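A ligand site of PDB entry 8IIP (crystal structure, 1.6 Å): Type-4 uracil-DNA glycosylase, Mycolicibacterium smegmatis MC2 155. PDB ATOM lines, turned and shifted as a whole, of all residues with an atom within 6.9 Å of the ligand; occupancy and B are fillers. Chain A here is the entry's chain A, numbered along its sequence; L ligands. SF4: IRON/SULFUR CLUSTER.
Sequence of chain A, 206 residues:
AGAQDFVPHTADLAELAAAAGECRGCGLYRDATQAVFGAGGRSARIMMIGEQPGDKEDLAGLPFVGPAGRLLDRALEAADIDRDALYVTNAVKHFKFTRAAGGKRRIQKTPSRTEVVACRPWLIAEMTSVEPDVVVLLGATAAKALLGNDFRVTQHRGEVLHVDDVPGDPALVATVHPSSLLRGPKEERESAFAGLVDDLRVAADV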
ATOM      1  N   GLY A   2       5.263  22.776  32.405  1.00  0.00           N
ATOM      2  CA  GLY A   2       4.472  22.523  31.200  1.00  0.00           C
ATOM      3  C   GLY A   2       2.987  22.717  31.390  1.00  0.00           C
ATOM      4  O   GLY A   2       2.574  23.736  31.926  1.00  0.00           O
ATOM      5  N   ALA A   3       2.214  21.744  30.909  1.00  0.00           N
ATOM      6  CA  ALA A   3       0.743  21.833  30.927  1.00  0.00           C
ATOM      7  C   ALA A   3       0.147  21.395  32.253  1.00  0.00           C
ATOM      8  O   ALA A   3      -1.037  21.522  32.394  1.00  0.00           O
ATOM      9  CB  ALA A   3       0.221  20.888  29.863  1.00  0.00           C
ATOM     10  N   PHE A   6      -2.723  23.282  33.942  1.00  0.00           N
ATOM     11  CA  PHE A   6      -3.900  23.532  33.087  1.00  0.00           C
ATOM     12  C   PHE A   6      -4.793  22.288  33.033  1.00  0.00           C
ATOM     13  O   PHE A   6      -5.891  22.408  32.544  1.00  0.00           O
ATOM     14  CB  PHE A   6      -3.422  23.929  31.688  1.00  0.00           C
ATOM     15  CG  PHE A   6      -2.669  25.222  31.633  1.00  0.00           C
ATOM     16  CD1 PHE A   6      -3.335  26.433  31.645  1.00  0.00           C
ATOM     17  CD2 PHE A   6      -1.284  25.239  31.553  1.00  0.00           C
ATOM     18  CE1 PHE A   6      -2.637  27.637  31.588  1.00  0.00           C
ATOM     19  CE2 PHE A   6      -0.590  26.433  31.508  1.00  0.00           C
ATOM     20  CZ  PHE A   6      -1.269  27.626  31.532  1.00  0.00           C
ATOM     21  N   ALA A  20      -8.039  21.829  27.727  1.00  0.00           N
ATOM     22  CA  ALA A  20      -6.916  21.926  26.802  1.00  0.00           C
ATOM     23  C   ALA A  20      -7.053  23.111  25.850  1.00  0.00           C
ATOM     24  O   ALA A  20      -6.035  23.677  25.427  1.00  0.00           O
ATOM     25  CB  ALA A  20      -6.758  20.613  26.024  1.00  0.00           C
ATOM     26  N   GLY A  21      -8.282  23.508  25.505  1.00  0.00           N
ATOM     27  CA  GLY A  21      -8.448  24.696  24.695  1.00  0.00           C
ATOM     28  C   GLY A  21      -7.859  25.942  25.337  1.00  0.00           C
ATOM     29  O   GLY A  21      -7.493  26.889  24.635  1.00  0.00           O
ATOM     30  N   GLU A  22      -7.715  25.906  26.657  1.00  0.00           N
ATOM     31  CA  GLU A  22      -7.173  27.070  27.418  1.00  0.00           C
ATOM     32  C   GLU A  22      -5.703  26.850  27.826  1.00  0.00           C
ATOM     33  O   GLU A  22      -5.180  27.692  28.524  1.00  0.00           O
ATOM     34  CB  GLU A  22      -7.992  27.277  28.700  1.00  0.00           C
ATOM     35  CG  GLU A  22      -9.474  27.062  28.509  1.00  0.00           C
ATOM     36  CD  GLU A  22     -10.219  28.357  28.269  1.00  0.00           C
ATOM     37  OE1 GLU A  22     -11.309  28.518  28.840  1.00  0.00           O
ATOM     38  OE2 GLU A  22      -9.704  29.199  27.519  1.00  0.00           O
ATOM     39  N   CYS A  23      -5.076  25.760  27.355  1.00  0.00           N
ATOM     40  CA  CYS A  23      -3.714  25.463  27.782  1.00  0.00           C
ATOM     41  C   CYS A  23      -2.733  26.455  27.194  1.00  0.00           C
ATOM     42  O   CYS A  23      -2.869  26.864  26.038  1.00  0.00           O
ATOM     43  CB  CYS A  23      -3.342  24.036  27.357  1.00  0.00           C
ATOM     44  SG  CYS A  23      -1.742  23.505  27.995  1.00  0.00           S
ATOM     45  N   ARG A  24      -1.751  26.878  28.016  1.00  0.00           N
ATOM     46  CA  ARG A  24      -0.607  27.667  27.581  1.00  0.00           C
ATOM     47  C   ARG A  24       0.696  26.992  28.026  1.00  0.00           C
ATOM     48  O   ARG A  24       1.709  27.669  28.230  1.00  0.00           O
ATOM     49  CB  ARG A  24      -0.685  29.095  28.131  1.00  0.00           C
ATOM     50  CG  ARG A  24      -2.001  29.802  27.804  1.00  0.00           C
ATOM     51  CD  ARG A  24      -1.962  31.298  28.164  1.00  0.00           C
ATOM     52  NE  ARG A  24      -1.486  31.531  29.530  1.00  0.00           N
ATOM     53  CZ  ARG A  24      -2.236  31.356  30.600  1.00  0.00           C
ATOM     54  NH1 ARG A  24      -3.511  30.985  30.507  1.00  0.00           N
ATOM     55  NH2 ARG A  24      -1.704  31.526  31.805  1.00  0.00           N
ATOM     56  N   GLY A  25       0.675  25.656  28.175  1.00  0.00           N
ATOM     57  CA  GLY A  25       1.797  24.890  28.716  1.00  0.00           C
ATOM     58  C   GLY A  25       3.067  24.974  27.901  1.00  0.00           C
ATOM     59  O   GLY A  25       4.161  24.670  28.423  1.00  0.00           O
ATOM     60  N   CYS A  26       2.961  25.343  26.636  1.00  0.00           N
ATOM     61  CA  CYS A  26       4.123  25.648  25.792  1.00  0.00           C
ATOM     62  C   CYS A  26       3.691  26.760  24.836  1.00  0.00           C
ATOM     63  O   CYS A  26       2.596  27.307  24.967  1.00  0.00           O
ATOM     64  CB  CYS A  26       4.629  24.367  25.117  1.00  0.00           C
ATOM     65  SG  CYS A  26       3.680  23.784  23.670  1.00  0.00           S
ATOM     66  N   GLY A  27       4.540  27.100  23.883  1.00  0.00           N
ATOM     67  CA  GLY A  27       4.184  28.208  23.009  1.00  0.00           C
ATOM     68  C   GLY A  27       3.261  27.874  21.849  1.00  0.00           C
ATOM     69  O   GLY A  27       2.853  28.783  21.117  1.00  0.00           O
ATOM     70  N   LEU A  28       2.911  26.598  21.665  1.00  0.00           N
ATOM     71  CA  LEU A  28       2.263  26.198  20.423  1.00  0.00           C
ATOM     72  C   LEU A  28       0.816  26.668  20.332  1.00  0.00           C
ATOM     73  O   LEU A  28       0.273  26.716  19.221  1.00  0.00           O
ATOM     74  CB  LEU A  28       2.338  24.674  20.265  1.00  0.00           C
ATOM     75  CG  LEU A  28       3.757  24.144  20.055  1.00  0.00           C
ATOM     76  CD1 LEU A  28       3.736  22.625  19.896  1.00  0.00           C
ATOM     77  CD2 LEU A  28       4.388  24.792  18.843  1.00  0.00           C
ATOM     78  N   TYR A  29       0.175  26.988  21.465  1.00  0.00           N
ATOM     79  CA  TYR A  29      -1.197  27.474  21.418  1.00  0.00           C
ATOM     80  C   TYR A  29      -1.334  28.792  20.667  1.00  0.00           C
ATOM     81  O   TYR A  29      -2.420  29.113  20.187  1.00  0.00           O
ATOM     82  CB  TYR A  29      -1.759  27.645  22.834  1.00  0.00           C
ATOM     83  CG  TYR A  29      -1.219  28.881  23.528  1.00  0.00           C
ATOM     84  CD1 TYR A  29       0.000  28.847  24.188  1.00  0.00           C
ATOM     85  CD2 TYR A  29      -1.933  30.087  23.525  1.00  0.00           C
ATOM     86  CE1 TYR A  29       0.511  29.972  24.806  1.00  0.00           C
ATOM     87  CE2 TYR A  29      -1.439  31.215  24.147  1.00  0.00           C
ATOM     88  CZ  TYR A  29      -0.214  31.145  24.787  1.00  0.00           C
ATOM     89  OH  TYR A  29       0.291  32.259  25.418  1.00  0.00           O
ATOM     90  N   ARG A  30      -0.256  29.574  20.597  1.00  0.00           N
ATOM     91  CA  ARG A  30      -0.394  30.938  20.020  1.00  0.00           C
ATOM     92  C   ARG A  30      -0.792  30.931  18.547  1.00  0.00           C
ATOM     93  O   ARG A  30      -1.732  31.621  18.203  1.00  0.00           O
ATOM     94  CB  ARG A  30       0.909  31.727  20.204  1.00  0.00           C
ATOM     95  CG  ARG A  30       1.356  31.895  21.644  1.00  0.00           C
ATOM     96  CD  ARG A  30       2.370  33.022  21.788  1.00  0.00           C
ATOM     97  NE  ARG A  30       3.112  32.975  23.035  1.00  0.00           N
ATOM     98  N   ALA A  35      -6.834  23.785  20.202  1.00  0.00           N
ATOM     99  CA  ALA A  35      -6.306  22.507  20.625  1.00  0.00           C
ATOM    100  C   ALA A  35      -7.080  21.404  19.929  1.00  0.00           C
ATOM    101  O   ALA A  35      -8.277  21.544  19.631  1.00  0.00           O
ATOM    102  CB  ALA A  35      -6.420  22.350  22.145  1.00  0.00           C
ATOM    103  N   ALA A  91       0.609  13.212  20.689  1.00  0.00           N
ATOM    104  CA  ALA A  91       1.521  13.582  21.780  1.00  0.00           C
ATOM    105  C   ALA A  91       1.436  15.073  22.087  1.00  0.00           C
ATOM    106  O   ALA A  91       1.570  15.491  23.253  1.00  0.00           O
ATOM    107  CB  ALA A  91       2.946  13.200  21.405  1.00  0.00           C
ATOM    108  N   VAL A  92       1.262  15.896  21.056  1.00  0.00           N
ATOM    109  CA  VAL A  92       1.147  17.345  21.189  1.00  0.00           C
ATOM    110  C   VAL A  92      -0.214  17.760  20.649  1.00  0.00           C
ATOM    111  O   VAL A  92      -0.679  17.201  19.653  1.00  0.00           O
ATOM    112  CB  VAL A  92       2.326  17.987  20.436  1.00  0.00           C
ATOM    113  CG1 VAL A  92       2.092  19.453  20.092  1.00  0.00           C
ATOM    114  CG2 VAL A  92       3.623  17.772  21.257  1.00  0.00           C
ATOM    115  N   LYS A  93      -0.892  18.701  21.347  1.00  0.00           N
ATOM    116  CA  LYS A  93      -2.290  19.056  21.066  1.00  0.00           C
ATOM    117  C   LYS A  93      -2.478  20.294  20.179  1.00  0.00           C
ATOM    118  O   LYS A  93      -3.606  20.552  19.747  1.00  0.00           O
ATOM    119  CB  LYS A  93      -3.078  19.301  22.369  1.00  0.00           C
ATOM    120  CG  LYS A  93      -3.895  18.139  22.924  1.00  0.00           C
ATOM    121  CD  LYS A  93      -3.071  16.898  23.076  1.00  0.00           C
ATOM    122  CE  LYS A  93      -3.854  15.799  23.832  1.00  0.00           C
ATOM    123  NZ  LYS A  93      -2.922  14.616  24.005  1.00  0.00           N
ATOM    124  N   HIS A  94      -1.420  21.041  19.936  1.00  0.00           N
ATOM    125  CA  HIS A  94      -1.505  22.221  19.048  1.00  0.00           C
ATOM    126  C   HIS A  94      -0.570  22.058  17.848  1.00  0.00           C
ATOM    127  O   HIS A  94       0.537  21.650  18.032  1.00  0.00           O
ATOM    128  CB  HIS A  94      -1.175  23.528  19.767  1.00  0.00           C
ATOM    129  CG  HIS A  94      -2.305  24.095  20.552  1.00  0.00           C
ATOM    130  ND1 HIS A  94      -2.386  23.963  21.900  1.00  0.00           N
ATOM    131  CD2 HIS A  94      -3.400  24.782  20.199  1.00  0.00           C
ATOM    132  CE1 HIS A  94      -3.453  24.551  22.370  1.00  0.00           C
ATOM    133  NE2 HIS A  94      -4.091  25.052  21.341  1.00  0.00           N
ATOM    134  N   PHE A  95      -1.105  22.405  16.704  1.00  0.00           N
ATOM    135  CA  PHE A  95      -0.373  22.282  15.443  1.00  0.00           C
ATOM    136  C   PHE A  95       0.827  23.227  15.410  1.00  0.00           C
ATOM    137  O   PHE A  95       0.669  24.428  15.615  1.00  0.00           O
ATOM    138  CB  PHE A  95      -1.360  22.614  14.320  1.00  0.00           C
ATOM    139  CG  PHE A  95      -0.835  22.561  12.910  1.00  0.00           C
ATOM    140  CD1 PHE A  95       0.064  21.581  12.490  1.00  0.00           C
ATOM    141  CD2 PHE A  95      -1.323  23.462  11.965  1.00  0.00           C
ATOM    142  CE1 PHE A  95       0.485  21.534  11.163  1.00  0.00           C
ATOM    143  CE2 PHE A  95      -0.913  23.411  10.646  1.00  0.00           C
ATOM    144  CZ  PHE A  95      -0.010  22.441  10.236  1.00  0.00           C
ATOM    145  N   GLU A 115       8.595  20.545  24.021  1.00  0.00           N
ATOM    146  CA  GLU A 115       7.153  20.668  23.818  1.00  0.00           C
ATOM    147  C   GLU A 115       6.436  19.355  24.100  1.00  0.00           C
ATOM    148  O   GLU A 115       5.335  19.346  24.665  1.00  0.00           O
ATOM    149  CB  GLU A 115       6.886  21.148  22.385  1.00  0.00           C
ATOM    150  CG  GLU A 115       7.257  22.617  22.219  1.00  0.00           C
ATOM    151  CD  GLU A 115       7.549  23.020  20.774  1.00  0.00           C
ATOM    152  OE1 GLU A 115       7.800  22.141  19.930  1.00  0.00           O
ATOM    153  OE2 GLU A 115       7.547  24.228  20.491  1.00  0.00           O
ATOM    154  N   VAL A 116       7.044  18.235  23.698  1.00  0.00           N
ATOM    155  CA  VAL A 116       6.434  16.938  23.980  1.00  0.00           C
ATOM    156  C   VAL A 116       6.300  16.729  25.487  1.00  0.00           C
ATOM    157  O   VAL A 116       5.252  16.312  25.986  1.00  0.00           O
ATOM    158  CB  VAL A 116       7.268  15.811  23.328  1.00  0.00           C
ATOM    159  CG1 VAL A 116       6.795  14.441  23.825  1.00  0.00           C
ATOM    160  CG2 VAL A 116       7.223  15.906  21.805  1.00  0.00           C
ATOM    161  N   VAL A 117       7.380  17.016  26.232  1.00  0.00           N
ATOM    162  CA  VAL A 117       7.314  16.826  27.679  1.00  0.00           C
ATOM    163  C   VAL A 117       6.326  17.797  28.303  1.00  0.00           C
ATOM    164  O   VAL A 117       5.580  17.447  29.240  1.00  0.00           O
ATOM    165  CB  VAL A 117       8.728  16.970  28.298  1.00  0.00           C
ATOM    166  CG1 VAL A 117       8.633  17.050  29.830  1.00  0.00           C
ATOM    167  CG2 VAL A 117       9.625  15.812  27.843  1.00  0.00           C
ATOM    168  N   ALA A 118       6.237  19.024  27.763  1.00  0.00           N
ATOM    169  CA  ALA A 118       5.281  19.998  28.276  1.00  0.00           C
ATOM    170  C   ALA A 118       3.842  19.517  28.104  1.00  0.00           C
ATOM    171  O   ALA A 118       3.001  19.727  28.991  1.00  0.00           O
ATOM    172  CB  ALA A 118       5.457  21.348  27.581  1.00  0.00           C
ATOM    173  N   CYS A 119       3.539  18.879  26.968  1.00  0.00           N
ATOM    174  CA  CYS A 119       2.171  18.464  26.691  1.00  0.00           C
ATOM    175  C   CYS A 119       1.819  17.113  27.291  1.00  0.00           C
ATOM    176  O   CYS A 119       0.624  16.768  27.396  1.00  0.00           O
ATOM    177  CB  CYS A 119       1.953  18.392  25.169  1.00  0.00           C
ATOM    178  SG  CYS A 119       0.218  18.670  24.650  1.00  0.00           S
ATOM    179  N   ARG A 120       2.818  16.334  27.694  1.00  0.00           N
ATOM    180  CA  ARG A 120       2.589  14.976  28.162  1.00  0.00           C
ATOM    181  C   ARG A 120       1.572  14.874  29.292  1.00  0.00           C
ATOM    182  O   ARG A 120       0.862  13.867  29.362  1.00  0.00           O
ATOM    183  CB  ARG A 120       3.910  14.329  28.583  1.00  0.00           C
ATOM    184  CG  ARG A 120       3.812  12.819  28.758  1.00  0.00           C
ATOM    185  CD  ARG A 120       5.184  12.205  28.711  1.00  0.00           C
ATOM    186  NE  ARG A 120       6.005  12.776  29.763  1.00  0.00           N
ATOM    187  CZ  ARG A 120       7.317  12.616  29.844  1.00  0.00           C
ATOM    188  NH1 ARG A 120       7.986  11.918  28.947  1.00  0.00           N
ATOM    189  NH2 ARG A 120       7.971  13.184  30.859  1.00  0.00           N
ATOM    190  N   PRO A 121       1.437  15.858  30.201  1.00  0.00           N
ATOM    191  CA  PRO A 121       0.342  15.753  31.194  1.00  0.00           C
ATOM    192  C   PRO A 121      -1.031  15.514  30.597  1.00  0.00           C
ATOM    193  O   PRO A 121      -1.849  14.863  31.248  1.00  0.00           O
ATOM    194  CB  PRO A 121       0.406  17.089  31.944  1.00  0.00           C
ATOM    195  CG  PRO A 121       1.845  17.504  31.837  1.00  0.00           C
ATOM    196  CD  PRO A 121       2.264  17.066  30.453  1.00  0.00           C
ATOM    197  N   TRP A 122      -1.327  16.036  29.395  1.00  0.00           N
ATOM    198  CA  TRP A 122      -2.609  15.710  28.767  1.00  0.00           C
ATOM    199  C   TRP A 122      -2.673  14.228  28.416  1.00  0.00           C
ATOM    200  O   TRP A 122      -3.686  13.566  28.671  1.00  0.00           O
ATOM    201  CB  TRP A 122      -2.856  16.562  27.525  1.00  0.00           C
ATOM    202  CG  TRP A 122      -3.030  17.998  27.862  1.00  0.00           C
ATOM    203  CD1 TRP A 122      -2.216  19.036  27.510  1.00  0.00           C
ATOM    204  CD2 TRP A 122      -4.122  18.571  28.605  1.00  0.00           C
ATOM    205  NE1 TRP A 122      -2.701  20.219  28.014  1.00  0.00           N
ATOM    206  CE2 TRP A 122      -3.879  19.966  28.681  1.00  0.00           C
ATOM    207  CE3 TRP A 122      -5.269  18.046  29.201  1.00  0.00           C
ATOM    208  CZ2 TRP A 122      -4.749  20.842  29.343  1.00  0.00           C
ATOM    209  CZ3 TRP A 122      -6.134  18.931  29.872  1.00  0.00           C
ATOM    210  CH2 TRP A 122      -5.857  20.303  29.934  1.00  0.00           C
HETATM  211 FE1  SF4 L   1       0.101  20.938  24.586  1.00  0.00          FE
HETATM  212 FE2  SF4 L   1       1.589  23.185  24.409  1.00  0.00          FE
HETATM  213 FE3  SF4 L   1      -0.601  23.074  26.012  1.00  0.00          FE
HETATM  214 FE4  SF4 L   1      -0.885  23.096  23.378  1.00  0.00          FE
HETATM  215  S1  SF4 L   1       0.010  24.813  24.656  1.00  0.00           S
HETATM  216  S2  SF4 L   1      -2.009  21.726  24.816  1.00  0.00           S
HETATM  217  S3  SF4 L   1       0.856  21.848  22.663  1.00  0.00           S
HETATM  218  S4  SF4 L   1       1.328  21.926  26.260  1.00  0.00           S
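The backbone NH (N) of His 94 sits close to a sulfur (S3) of the ligand (3.6 Å).
A ring nitrogen (ND1) of His 94 is bound to an iron atom (FE4) of the ligand, at 2.3 Å.
FE1 of the ligand is bound by SG of Cys 119 (2.3 Å).
FE3 of the ligand is bound by SG of Cys 23 (2.3 Å).
The side-chain sulfur (SG) of Cys 26 binds an iron atom (FE2) of the ligand, 2.3 Å away.
N of Cys 26 lies close to S1 of the ligand, at 3.6 Å.
The indole nitrogen of Trp 122 lies close to a sulfur (S2) of the ligand (3.6 Å).
The backbone NH (N) of Gly 25 lies close to a sulfur (S1) of the ligand (3.7 Å).
Residues that only touch the ligand: Lys 93, Val 92, Tyr 29, Ala 118, Ala 3 and Leu 28.
Hydrophobic or aromatic side chains within 4 Å of the ligand: Ala 3, Leu 28, Tyr 29, Val 92, His 94 and Trp 122.
The nearest printed residue that does not touch the ligand is Arg 24 (4.1 Å).
The side-chain sulfur (SG) of Cys 119 lies close to the backbone carbonyl oxygen (O) of Ala 91.
The backbone carbonyl oxygen (O) of Ala 118 lies within hydrogen-bond range of the backbone NH (N) of Ala 3.
N of Lys 93 sits close to SG of Cys 119 (3.5 Å).
The side-chain sulfur of Cys 26 lies close to the backbone NH of Leu 28, at 3.5 Å.
The backbone NH (N) of Ala 35 sits at hydrogen-bond distance from a ring nitrogen (NE2) of His 94.
The side-chain sulfur (SG) of Cys 23 lies close to the backbone NH (N) of Gly 25, 3.2 Å away.
The side-chain sulfur (SG) of Cys 23 lies close to the indole nitrogen (NE1) of Trp 122, 3.4 Å away.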
